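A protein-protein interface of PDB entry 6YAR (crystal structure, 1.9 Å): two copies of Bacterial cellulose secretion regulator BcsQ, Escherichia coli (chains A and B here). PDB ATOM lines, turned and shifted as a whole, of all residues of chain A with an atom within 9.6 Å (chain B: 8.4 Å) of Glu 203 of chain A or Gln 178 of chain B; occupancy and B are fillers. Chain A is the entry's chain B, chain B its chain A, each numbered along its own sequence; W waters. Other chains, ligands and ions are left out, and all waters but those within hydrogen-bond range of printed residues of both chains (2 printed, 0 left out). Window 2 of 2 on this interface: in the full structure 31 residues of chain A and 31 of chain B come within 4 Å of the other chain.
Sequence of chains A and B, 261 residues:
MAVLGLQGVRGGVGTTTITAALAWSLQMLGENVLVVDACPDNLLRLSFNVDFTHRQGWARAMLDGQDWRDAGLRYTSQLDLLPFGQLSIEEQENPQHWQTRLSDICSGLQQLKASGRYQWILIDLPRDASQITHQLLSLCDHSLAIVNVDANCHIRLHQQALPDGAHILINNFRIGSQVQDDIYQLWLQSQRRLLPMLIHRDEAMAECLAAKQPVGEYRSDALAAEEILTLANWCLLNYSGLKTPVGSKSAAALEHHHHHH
Of the printed residues of chain B, Glu 203 of chain A touches Ser 177, Gln 178 and Val 179.
Of the printed residues of chain B, Ala 206 of chain A touches Val 179.
Of the printed residues of chain B, Ala 210 of chain A touches Val 179.
Val 215 of chain A touches none of the printed residues of chain B.
Of the printed residues of chain A, Gln 178 of chain B touches Glu 203.
Of the printed residues of chain A, Gln 180 of chain B touches Arg 201.
The nearest printed residue of chain A that does not touch Gln 178 of chain B is Glu 207 of chain A (4.5 Å).
The nearest printed residue of chain A that does not touch Val 179 of chain B is Cys 208 of chain A (6.5 Å).
The side-chain carboxylate of Glu 203 of chain A sits at hydrogen-bond distance from the side-chain hydroxyl of Ser 177 of chain B (2.7 Å).
OE2 of Glu 203 of chain A sits at hydrogen-bond distance from N of Gln 178 of chain B, at 3.4 Å.
N of Val 179 of chain B sits at hydrogen-bond distance from OE2 of Glu 203 of chain A, at 3.3 Å.
OE1 of Gln 180 of chain B sits at hydrogen-bond distance from NH2 of Arg 201 of chain A, 3.0 Å away.
The side-chain hydroxyl of Ser 177 of chain B sits close to the backbone NH of Gln 180 of chain B.
OE1 of Gln 178 of chain B lies close to OD1 of Asp 182 of chain B.
The side-chain amide oxygen (OD1) of Asn 172 of chain A lies within hydrogen-bond range of the guanidinium group (NH1) of Arg 201 of chain A.
The backbone carbonyl oxygen of Phe 173 of chain A is in hydrogen-bond range of the backbone NH of Arg 201 of chain A.
The side-chain carboxylate of Glu 207 of chain A lies within hydrogen-bond range of the side-chain hydroxyl of Tyr 218 of chain A (2.4 Å).
The guanidinium group (NH1) of Arg 219 of chain A is in salt-bridge range of the side-chain carboxylate (OE1) of Glu 207 of chain A (3.1 Å).
Water W1 lies within hydrogen-bond range of the side-chain amide oxygen of Gln 180 of chain B and the guanidinium group of Arg 201 of chain A.
Water W2 bridges the backbone NH (N) of Gln 178 of chain B (2.9 Å) and the side-chain carboxylate (OE2) of Glu 203 of chain A (3.3 Å).
Printed residues of chain B that touch a printed residue of chain A: Ser 177, Gln 178, Val 179 and Gln 180.
No position is printed for both chains.
Of the 7 pairs that touch across the chains among the printed residues, none has its exchanged pair printed and touching as well.
CB of Ala 206 of chain A touches CG1 of Val 179 of chain B (3.8 Å).
CG of Glu 207 of chain A touches CG1 of Val 179 of chain B, at 3.8 Å.
CG2 of Val 179 of chain B touches CB of Ala 210 of chain A, 3.7 Å away.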
ATOM      1  N   THR A  17      -3.760  37.388  13.736  1.00  0.00           N
ATOM      2  CA  THR A  17      -2.616  37.025  12.918  1.00  0.00           C
ATOM      3  C   THR A  17      -2.383  38.071  11.842  1.00  0.00           C
ATOM      4  O   THR A  17      -1.239  38.396  11.529  1.00  0.00           O
ATOM      5  CB  THR A  17      -2.840  35.644  12.286  1.00  0.00           C
ATOM      6  OG1 THR A  17      -3.231  34.705  13.301  1.00  0.00           O
ATOM      7  CG2 THR A  17      -1.565  35.150  11.614  1.00  0.00           C
ATOM      8  N   ASN A 172      -8.347  33.298   4.851  1.00  0.00           N
ATOM      9  CA  ASN A 172      -8.599  31.853   4.832  1.00  0.00           C
ATOM     10  C   ASN A 172      -9.231  31.358   3.527  1.00  0.00           C
ATOM     11  O   ASN A 172      -9.886  30.308   3.521  1.00  0.00           O
ATOM     12  CB  ASN A 172      -9.481  31.402   6.015  1.00  0.00           C
ATOM     13  CG  ASN A 172      -8.710  31.287   7.313  1.00  0.00           C
ATOM     14  OD1 ASN A 172      -7.548  30.898   7.314  1.00  0.00           O
ATOM     15  ND2 ASN A 172      -9.373  31.592   8.442  1.00  0.00           N
ATOM     16  N   PHE A 173      -9.071  32.082   2.420  1.00  0.00           N
ATOM     17  CA  PHE A 173      -9.636  31.620   1.156  1.00  0.00           C
ATOM     18  C   PHE A 173      -8.927  30.338   0.737  1.00  0.00           C
ATOM     19  O   PHE A 173      -7.697  30.257   0.794  1.00  0.00           O
ATOM     20  CB  PHE A 173      -9.484  32.706   0.085  1.00  0.00           C
ATOM     21  CG  PHE A 173     -10.430  32.556  -1.075  1.00  0.00           C
ATOM     22  CD1 PHE A 173     -11.752  32.960  -0.969  1.00  0.00           C
ATOM     23  CD2 PHE A 173     -10.002  32.008  -2.271  1.00  0.00           C
ATOM     24  CE1 PHE A 173     -12.631  32.815  -2.045  1.00  0.00           C
ATOM     25  CE2 PHE A 173     -10.878  31.852  -3.347  1.00  0.00           C
ATOM     26  CZ  PHE A 173     -12.183  32.265  -3.239  1.00  0.00           C
ATOM     27  N   ILE A 199      -6.459  37.104   1.483  1.00  0.00           N
ATOM     28  CA  ILE A 199      -5.438  36.217   2.027  1.00  0.00           C
ATOM     29  C   ILE A 199      -5.962  34.792   1.955  1.00  0.00           C
ATOM     30  O   ILE A 199      -7.069  34.508   2.432  1.00  0.00           O
ATOM     31  CB  ILE A 199      -5.090  36.575   3.477  1.00  0.00           C
ATOM     32  CG1 ILE A 199      -4.895  38.076   3.609  1.00  0.00           C
ATOM     33  CG2 ILE A 199      -3.867  35.804   3.952  1.00  0.00           C
ATOM     34  CD1 ILE A 199      -5.130  38.555   5.007  1.00  0.00           C
ATOM     35  N   HIS A 200      -5.164  33.899   1.368  1.00  0.00           N
ATOM     36  CA  HIS A 200      -5.497  32.485   1.329  1.00  0.00           C
ATOM     37  C   HIS A 200      -5.185  31.804   2.655  1.00  0.00           C
ATOM     38  O   HIS A 200      -4.313  32.239   3.416  1.00  0.00           O
ATOM     39  CB  HIS A 200      -4.716  31.771   0.218  1.00  0.00           C
ATOM     40  CG  HIS A 200      -5.224  32.066  -1.154  1.00  0.00           C
ATOM     41  ND1 HIS A 200      -4.897  33.220  -1.836  1.00  0.00           N
ATOM     42  CD2 HIS A 200      -6.039  31.361  -1.970  1.00  0.00           C
ATOM     43  CE1 HIS A 200      -5.500  33.216  -3.012  1.00  0.00           C
ATOM     44  NE2 HIS A 200      -6.187  32.093  -3.123  1.00  0.00           N
ATOM     45  N   ARG A 201      -5.904  30.711   2.916  1.00  0.00           N
ATOM     46  CA  ARG A 201      -5.404  29.702   3.839  1.00  0.00           C
ATOM     47  C   ARG A 201      -3.992  29.324   3.417  1.00  0.00           C
ATOM     48  O   ARG A 201      -3.742  29.041   2.244  1.00  0.00           O
ATOM     49  CB  ARG A 201      -6.314  28.471   3.818  1.00  0.00           C
ATOM     50  CG  ARG A 201      -6.055  27.467   4.940  1.00  0.00           C
ATOM     51  CD  ARG A 201      -6.702  27.956   6.236  1.00  0.00           C
ATOM     52  NE  ARG A 201      -6.530  27.021   7.348  1.00  0.00           N
ATOM     53  CZ  ARG A 201      -6.820  27.302   8.610  1.00  0.00           C
ATOM     54  NH1 ARG A 201      -7.299  28.493   8.937  1.00  0.00           N
ATOM     55  NH2 ARG A 201      -6.625  26.390   9.550  1.00  0.00           N
ATOM     56  N   ASP A 202      -3.067  29.312   4.367  1.00  0.00           N
ATOM     57  CA  ASP A 202      -1.668  29.164   4.002  1.00  0.00           C
ATOM     58  C   ASP A 202      -0.961  28.587   5.212  1.00  0.00           C
ATOM     59  O   ASP A 202      -1.113  29.115   6.312  1.00  0.00           O
ATOM     60  CB  ASP A 202      -1.092  30.544   3.587  1.00  0.00           C
ATOM     61  CG  ASP A 202       0.352  30.491   3.076  1.00  0.00           C
ATOM     62  OD1 ASP A 202       1.207  29.789   3.657  1.00  0.00           O
ATOM     63  OD2 ASP A 202       0.645  31.224   2.101  1.00  0.00           O
ATOM     64  N   GLU A 203      -0.192  27.515   5.009  1.00  0.00           N
ATOM     65  CA  GLU A 203       0.492  26.869   6.128  1.00  0.00           C
ATOM     66  C   GLU A 203       1.363  27.850   6.921  1.00  0.00           C
ATOM     67  O   GLU A 203       1.559  27.654   8.125  1.00  0.00           O
ATOM     68  CB  GLU A 203       1.329  25.690   5.612  1.00  0.00           C
ATOM     69  CG  GLU A 203       2.137  24.930   6.671  1.00  0.00           C
ATOM     70  CD  GLU A 203       1.292  24.043   7.618  1.00  0.00           C
ATOM     71  OE1 GLU A 203       0.088  23.802   7.341  1.00  0.00           O
ATOM     72  OE2 GLU A 203       1.851  23.567   8.637  1.00  0.00           O
ATOM     73  N   ALA A 204       1.876  28.913   6.281  1.00  0.00           N
ATOM     74  CA  ALA A 204       2.701  29.887   7.006  1.00  0.00           C
ATOM     75  C   ALA A 204       1.893  30.681   8.029  1.00  0.00           C
ATOM     76  O   ALA A 204       2.434  31.078   9.071  1.00  0.00           O
ATOM     77  CB  ALA A 204       3.383  30.860   6.038  1.00  0.00           C
ATOM     78  N   MET A 205       0.619  30.955   7.740  1.00  0.00           N
ATOM     79  CA  MET A 205      -0.264  31.660   8.670  1.00  0.00           C
ATOM     80  C   MET A 205      -0.678  30.766   9.831  1.00  0.00           C
ATOM     81  O   MET A 205      -1.101  31.253  10.886  1.00  0.00           O
ATOM     82  CB  MET A 205      -1.521  32.174   7.959  1.00  0.00           C
ATOM     83  CG  MET A 205      -1.277  33.230   6.880  1.00  0.00           C
ATOM     84  SD  MET A 205      -0.949  34.983   7.709  1.00  0.00           S
ATOM     85  CE  MET A 205      -2.822  35.436   8.191  1.00  0.00           C
ATOM     86  N   ALA A 206      -0.600  29.453   9.620  1.00  0.00           N
ATOM     87  CA  ALA A 206      -0.894  28.517  10.701  1.00  0.00           C
ATOM     88  C   ALA A 206       0.338  28.307  11.567  1.00  0.00           C
ATOM     89  O   ALA A 206       0.227  28.160  12.787  1.00  0.00           O
ATOM     90  CB  ALA A 206      -1.384  27.168  10.135  1.00  0.00           C
ATOM     91  N   GLU A 207       1.522  28.305  10.946  1.00  0.00           N
ATOM     92  CA  GLU A 207       2.752  28.016  11.669  1.00  0.00           C
ATOM     93  C   GLU A 207       3.316  29.233  12.398  1.00  0.00           C
ATOM     94  O   GLU A 207       4.007  29.070  13.409  1.00  0.00           O
ATOM     95  CB  GLU A 207       3.818  27.483  10.709  1.00  0.00           C
ATOM     96  CG  GLU A 207       3.477  26.118  10.044  1.00  0.00           C
ATOM     97  CD  GLU A 207       4.554  25.702   9.066  1.00  0.00           C
ATOM     98  OE1 GLU A 207       5.509  26.491   8.838  1.00  0.00           O
ATOM     99  OE2 GLU A 207       4.453  24.588   8.530  1.00  0.00           O
ATOM    100  N   CYS A 208       3.094  30.445  11.889  1.00  0.00           N
ATOM    101  CA  CYS A 208       3.831  31.584  12.438  1.00  0.00           C
ATOM    102  C   CYS A 208       3.458  31.842  13.899  1.00  0.00           C
ATOM    103  O   CYS A 208       4.323  32.225  14.693  1.00  0.00           O
ATOM    104  CB  CYS A 208       3.617  32.833  11.577  1.00  0.00           C
ATOM    105  SG  CYS A 208       1.900  33.321  11.350  1.00  0.00           S
ATOM    106  N   LEU A 209       2.199  31.589  14.281  1.00  0.00           N
ATOM    107  CA  LEU A 209       1.818  31.727  15.688  1.00  0.00           C
ATOM    108  C   LEU A 209       2.514  30.682  16.556  1.00  0.00           C
ATOM    109  O   LEU A 209       2.953  30.987  17.669  1.00  0.00           O
ATOM    110  CB  LEU A 209       0.299  31.627  15.841  1.00  0.00           C
ATOM    111  CG  LEU A 209      -0.245  31.731  17.266  1.00  0.00           C
ATOM    112  CD1 LEU A 209       0.320  32.995  17.941  1.00  0.00           C
ATOM    113  CD2 LEU A 209      -1.766  31.755  17.246  1.00  0.00           C
ATOM    114  N   ALA A 210       2.637  29.448  16.064  1.00  0.00           N
ATOM    115  CA  ALA A 210       3.379  28.437  16.809  1.00  0.00           C
ATOM    116  C   ALA A 210       4.872  28.749  16.870  1.00  0.00           C
ATOM    117  O   ALA A 210       5.555  28.270  17.780  1.00  0.00           O
ATOM    118  CB  ALA A 210       3.149  27.054  16.201  1.00  0.00           C
ATOM    119  N   ALA A 211       5.395  29.530  15.924  1.00  0.00           N
ATOM    120  CA  ALA A 211       6.769  30.010  15.978  1.00  0.00           C
ATOM    121  C   ALA A 211       6.886  31.355  16.683  1.00  0.00           C
ATOM    122  O   ALA A 211       7.996  31.878  16.805  1.00  0.00           O
ATOM    123  CB  ALA A 211       7.355  30.132  14.569  1.00  0.00           C
ATOM    124  N   VAL A 215       3.920  36.660  10.315  1.00  0.00           N
ATOM    125  CA  VAL A 215       4.097  35.759   9.173  1.00  0.00           C
ATOM    126  C   VAL A 215       5.247  36.230   8.285  1.00  0.00           C
ATOM    127  O   VAL A 215       6.012  35.412   7.760  1.00  0.00           O
ATOM    128  CB  VAL A 215       2.784  35.619   8.375  1.00  0.00           C
ATOM    129  CG1 VAL A 215       2.570  36.804   7.435  1.00  0.00           C
ATOM    130  CG2 VAL A 215       2.789  34.307   7.576  1.00  0.00           C
ATOM    131  N   TYR A 218       8.499  35.264   9.834  1.00  0.00           N
ATOM    132  CA  TYR A 218       8.651  33.814   9.903  1.00  0.00           C
ATOM    133  C   TYR A 218       9.025  33.223   8.540  1.00  0.00           C
ATOM    134  O   TYR A 218       9.943  32.393   8.436  1.00  0.00           O
ATOM    135  CB  TYR A 218       7.349  33.200  10.452  1.00  0.00           C
ATOM    136  CG  TYR A 218       7.325  31.705  10.392  1.00  0.00           C
ATOM    137  CD1 TYR A 218       8.158  30.939  11.206  1.00  0.00           C
ATOM    138  CD2 TYR A 218       6.465  31.040   9.521  1.00  0.00           C
ATOM    139  CE1 TYR A 218       8.142  29.541  11.135  1.00  0.00           C
ATOM    140  CE2 TYR A 218       6.457  29.667   9.439  1.00  0.00           C
ATOM    141  CZ  TYR A 218       7.291  28.919  10.243  1.00  0.00           C
ATOM    142  OH  TYR A 218       7.254  27.540  10.138  1.00  0.00           O
ATOM    143  N   ARG A 219       8.337  33.652   7.477  1.00  0.00           N
ATOM    144  CA  ARG A 219       8.611  33.183   6.114  1.00  0.00           C
ATOM    145  C   ARG A 219       8.384  34.376   5.182  1.00  0.00           C
ATOM    146  O   ARG A 219       7.261  34.613   4.727  1.00  0.00           O
ATOM    147  CB  ARG A 219       7.722  31.992   5.756  1.00  0.00           C
ATOM    148  CG  ARG A 219       8.305  31.036   4.703  1.00  0.00           C
ATOM    149  CD  ARG A 219       8.017  29.573   5.064  1.00  0.00           C
ATOM    150  NE  ARG A 219       6.662  29.153   4.715  1.00  0.00           N
ATOM    151  CZ  ARG A 219       6.060  28.061   5.185  1.00  0.00           C
ATOM    152  NH1 ARG A 219       6.675  27.264   6.049  1.00  0.00           N
ATOM    153  NH2 ARG A 219       4.826  27.782   4.807  1.00  0.00           N
ATOM    154  N   ALA A 222       6.668  33.596   1.974  1.00  0.00           N
ATOM    155  CA  ALA A 222       5.394  32.889   1.965  1.00  0.00           C
ATOM    156  C   ALA A 222       4.398  33.642   1.091  1.00  0.00           C
ATOM    157  O   ALA A 222       4.382  34.874   1.062  1.00  0.00           O
ATOM    158  CB  ALA A 222       4.849  32.747   3.384  1.00  0.00           C
ATOM    159  N   LEU A 223       3.572  32.897   0.357  1.00  0.00           N
ATOM    160  CA  LEU A 223       2.517  33.540  -0.421  1.00  0.00           C
ATOM    161  C   LEU A 223       1.657  34.452   0.462  1.00  0.00           C
ATOM    162  O   LEU A 223       1.317  35.573   0.066  1.00  0.00           O
ATOM    163  CB  LEU A 223       1.670  32.469  -1.125  1.00  0.00           C
ATOM    164  CG  LEU A 223       2.447  31.688  -2.200  1.00  0.00           C
ATOM    165  CD1 LEU A 223       1.626  30.574  -2.851  1.00  0.00           C
ATOM    166  CD2 LEU A 223       2.991  32.636  -3.270  1.00  0.00           C
ATOM    167  N   ALA A 224       1.326  34.003   1.679  1.00  0.00           N
ATOM    168  CA  ALA A 224       0.513  34.832   2.573  1.00  0.00           C
ATOM    169  C   ALA A 224       1.257  36.097   3.025  1.00  0.00           C
ATOM    170  O   ALA A 224       0.637  37.156   3.199  1.00  0.00           O
ATOM    171  CB  ALA A 224       0.056  34.017   3.787  1.00  0.00           C
ATOM    172  N   ALA A 225       2.579  36.012   3.225  1.00  0.00           N
ATOM    173  CA  ALA A 225       3.358  37.219   3.510  1.00  0.00           C
ATOM    174  C   ALA A 225       3.293  38.206   2.343  1.00  0.00           C
ATOM    175  O   ALA A 225       3.161  39.414   2.554  1.00  0.00           O
ATOM    176  CB  ALA A 225       4.815  36.862   3.823  1.00  0.00           C
ATOM    177  N   GLU A 227       0.754  38.386   0.230  1.00  0.00           N
ATOM    178  CA  GLU A 227      -0.606  38.915   0.229  1.00  0.00           C
ATOM    179  C   GLU A 227      -0.763  40.016   1.274  1.00  0.00           C
ATOM    180  O   GLU A 227      -1.415  41.036   1.021  1.00  0.00           O
ATOM    181  CB  GLU A 227      -1.609  37.777   0.456  1.00  0.00           C
ATOM    182  CG  GLU A 227      -1.595  36.752  -0.709  1.00  0.00           C
ATOM    183  CD  GLU A 227      -2.508  35.538  -0.522  1.00  0.00           C
ATOM    184  OE1 GLU A 227      -2.552  34.959   0.587  1.00  0.00           O
ATOM    185  OE2 GLU A 227      -3.161  35.143  -1.518  1.00  0.00           O
ATOM    186  N   VAL B 149      -8.254  22.349  15.588  1.00  0.00           N
ATOM    187  CA  VAL B 149      -6.855  22.055  15.867  1.00  0.00           C
ATOM    188  C   VAL B 149      -6.009  23.165  15.259  1.00  0.00           C
ATOM    189  O   VAL B 149      -5.639  23.111  14.076  1.00  0.00           O
ATOM    190  CB  VAL B 149      -6.419  20.681  15.327  1.00  0.00           C
ATOM    191  CG1 VAL B 149      -5.047  20.335  15.876  1.00  0.00           C
ATOM    192  CG2 VAL B 149      -7.441  19.592  15.682  1.00  0.00           C
ATOM    193  N   ARG B 174      -8.610  18.160   9.380  1.00  0.00           N
ATOM    194  CA  ARG B 174      -8.150  17.553   8.133  1.00  0.00           C
ATOM    195  C   ARG B 174      -6.643  17.404   8.234  1.00  0.00           C
ATOM    196  O   ARG B 174      -5.947  18.391   8.494  1.00  0.00           O
ATOM    197  CB  ARG B 174      -8.537  18.419   6.932  1.00  0.00           C
ATOM    198  CG  ARG B 174      -8.205  17.801   5.574  1.00  0.00           C
ATOM    199  CD  ARG B 174      -8.625  18.713   4.419  1.00  0.00           C
ATOM    200  NE  ARG B 174      -8.563  18.004   3.144  1.00  0.00           N
ATOM    201  CZ  ARG B 174      -9.604  17.429   2.547  1.00  0.00           C
ATOM    202  NH1 ARG B 174     -10.806  17.492   3.109  1.00  0.00           N
ATOM    203  NH2 ARG B 174      -9.444  16.796   1.383  1.00  0.00           N
ATOM    204  N   ILE B 175      -6.134  16.184   8.052  1.00  0.00           N
ATOM    205  CA  ILE B 175      -4.692  15.988   8.184  1.00  0.00           C
ATOM    206  C   ILE B 175      -3.987  16.576   6.968  1.00  0.00           C
ATOM    207  O   ILE B 175      -4.592  16.837   5.926  1.00  0.00           O
ATOM    208  CB  ILE B 175      -4.318  14.508   8.369  1.00  0.00           C
ATOM    209  CG1 ILE B 175      -4.508  13.750   7.063  1.00  0.00           C
ATOM    210  CG2 ILE B 175      -5.123  13.897   9.495  1.00  0.00           C
ATOM    211  CD1 ILE B 175      -3.965  12.339   7.104  1.00  0.00           C
ATOM    212  N   GLY B 176      -2.685  16.800   7.117  1.00  0.00           N
ATOM    213  CA  GLY B 176      -1.899  17.390   6.051  1.00  0.00           C
ATOM    214  C   GLY B 176      -1.079  18.583   6.494  1.00  0.00           C
ATOM    215  O   GLY B 176      -0.025  18.850   5.919  1.00  0.00           O
ATOM    216  N   SER B 177      -1.547  19.315   7.506  1.00  0.00           N
ATOM    217  CA  SER B 177      -0.829  20.462   8.039  1.00  0.00           C
ATOM    218  C   SER B 177       0.161  19.986   9.097  1.00  0.00           C
ATOM    219  O   SER B 177      -0.243  19.395  10.103  1.00  0.00           O
ATOM    220  CB  SER B 177      -1.809  21.473   8.630  1.00  0.00           C
ATOM    221  OG  SER B 177      -1.136  22.513   9.341  1.00  0.00           O
ATOM    222  N   GLN B 178       1.457  20.240   8.872  1.00  0.00           N
ATOM    223  CA  GLN B 178       2.464  19.813   9.842  1.00  0.00           C
ATOM    224  C   GLN B 178       2.160  20.349  11.244  1.00  0.00           C
ATOM    225  O   GLN B 178       2.235  19.608  12.232  1.00  0.00           O
ATOM    226  CB  GLN B 178       3.854  20.261   9.396  1.00  0.00           C
ATOM    227  CG  GLN B 178       4.953  19.859  10.368  1.00  0.00           C
ATOM    228  CD  GLN B 178       5.088  18.352  10.506  1.00  0.00           C
ATOM    229  OE1 GLN B 178       4.855  17.789  11.577  1.00  0.00           O
ATOM    230  NE2 GLN B 178       5.472  17.692   9.424  1.00  0.00           N
ATOM    231  N   VAL B 179       1.827  21.635  11.353  1.00  0.00           N
ATOM    232  CA  VAL B 179       1.659  22.230  12.677  1.00  0.00           C
ATOM    233  C   VAL B 179       0.360  21.742  13.325  1.00  0.00           C
ATOM    234  O   VAL B 179       0.340  21.372  14.504  1.00  0.00           O
ATOM    235  CB  VAL B 179       1.756  23.773  12.596  1.00  0.00           C
ATOM    236  CG1 VAL B 179       0.599  24.404  11.816  1.00  0.00           C
ATOM    237  CG2 VAL B 179       1.837  24.375  13.999  1.00  0.00           C
ATOM    238  N   GLN B 180      -0.724  21.666  12.553  1.00  0.00           N
ATOM    239  CA  GLN B 180      -1.984  21.168  13.097  1.00  0.00           C
ATOM    240  C   GLN B 180      -1.882  19.699  13.494  1.00  0.00           C
ATOM    241  O   GLN B 180      -2.403  19.300  14.542  1.00  0.00           O
ATOM    242  CB  GLN B 180      -3.100  21.410  12.085  1.00  0.00           C
ATOM    243  CG  GLN B 180      -3.233  22.907  11.774  1.00  0.00           C
ATOM    244  CD  GLN B 180      -4.293  23.220  10.741  1.00  0.00           C
ATOM    245  OE1 GLN B 180      -4.604  24.385  10.497  1.00  0.00           O
ATOM    246  NE2 GLN B 180      -4.847  22.190  10.121  1.00  0.00           N
ATOM    247  N   ASP B 181      -1.188  18.879  12.698  1.00  0.00           N
ATOM    248  CA  ASP B 181      -0.995  17.483  13.091  1.00  0.00           C
ATOM    249  C   ASP B 181      -0.121  17.371  14.337  1.00  0.00           C
ATOM    250  O   ASP B 181      -0.332  16.481  15.171  1.00  0.00           O
ATOM    251  CB  ASP B 181      -0.387  16.680  11.938  1.00  0.00           C
ATOM    252  CG  ASP B 181      -1.278  16.654  10.708  1.00  0.00           C
ATOM    253  OD1 ASP B 181      -2.498  16.898  10.842  1.00  0.00           O
ATOM    254  OD2 ASP B 181      -0.753  16.401   9.608  1.00  0.00           O
ATOM    255  N   ASP B 182       0.873  18.256  14.475  1.00  0.00           N
ATOM    256  CA  ASP B 182       1.702  18.271  15.678  1.00  0.00           C
ATOM    257  C   ASP B 182       0.870  18.610  16.912  1.00  0.00           C
ATOM    258  O   ASP B 182       0.962  17.929  17.941  1.00  0.00           O
ATOM    259  CB  ASP B 182       2.849  19.271  15.518  1.00  0.00           C
ATOM    260  CG  ASP B 182       3.936  18.778  14.568  1.00  0.00           C
ATOM    261  OD1 ASP B 182       3.951  17.569  14.235  1.00  0.00           O
ATOM    262  OD2 ASP B 182       4.769  19.606  14.146  1.00  0.00           O
ATOM    263  N   ILE B 183       0.050  19.658  16.820  1.00  0.00           N
ATOM    264  CA  ILE B 183      -0.868  19.991  17.906  1.00  0.00           C
ATOM    265  C   ILE B 183      -1.813  18.821  18.186  1.00  0.00           C
ATOM    266  O   ILE B 183      -2.013  18.421  19.338  1.00  0.00           O
ATOM    267  CB  ILE B 183      -1.644  21.279  17.573  1.00  0.00           C
ATOM    268  CG1 ILE B 183      -0.700  22.479  17.554  1.00  0.00           C
ATOM    269  CG2 ILE B 183      -2.777  21.487  18.588  1.00  0.00           C
ATOM    270  CD1 ILE B 183      -1.287  23.716  16.885  1.00  0.00           C
ATOM    271  N   TYR B 184      -2.400  18.248  17.130  1.00  0.00           N
ATOM    272  CA  TYR B 184      -3.345  17.151  17.314  1.00  0.00           C
ATOM    273  C   TYR B 184      -2.706  15.998  18.083  1.00  0.00           C
ATOM    274  O   TYR B 184      -3.230  15.566  19.117  1.00  0.00           O
ATOM    275  CB  TYR B 184      -3.880  16.683  15.959  1.00  0.00           C
ATOM    276  CG  TYR B 184      -4.742  15.438  16.038  1.00  0.00           C
ATOM    277  CD1 TYR B 184      -6.030  15.495  16.559  1.00  0.00           C
ATOM    278  CD2 TYR B 184      -4.271  14.209  15.591  1.00  0.00           C
ATOM    279  CE1 TYR B 184      -6.825  14.373  16.642  1.00  0.00           C
ATOM    280  CE2 TYR B 184      -5.070  13.061  15.674  1.00  0.00           C
ATOM    281  CZ  TYR B 184      -6.348  13.159  16.205  1.00  0.00           C
ATOM    282  OH  TYR B 184      -7.165  12.049  16.297  1.00  0.00           O
ATOM    283  N   GLN B 185      -1.557  15.500  17.612  1.00  0.00           N
ATOM    284  CA  GLN B 185      -0.871  14.432  18.339  1.00  0.00           C
ATOM    285  C   GLN B 185      -0.536  14.850  19.766  1.00  0.00           C
ATOM    286  O   GLN B 185      -0.566  14.018  20.682  1.00  0.00           O
ATOM    287  CB  GLN B 185       0.405  14.015  17.601  1.00  0.00           C
ATOM    288  CG  GLN B 185       0.165  13.364  16.238  1.00  0.00           C
ATOM    289  CD  GLN B 185      -0.607  12.053  16.324  1.00  0.00           C
ATOM    290  OE1 GLN B 185      -0.294  11.180  17.140  1.00  0.00           O
ATOM    291  NE2 GLN B 185      -1.620  11.910  15.475  1.00  0.00           N
HETATM  292  O   HOH W   1      -4.203  26.879  11.546  1.00  0.00           O
HETATM  293  O   HOH W   2       2.553  21.248   6.423  1.00  0.00           O
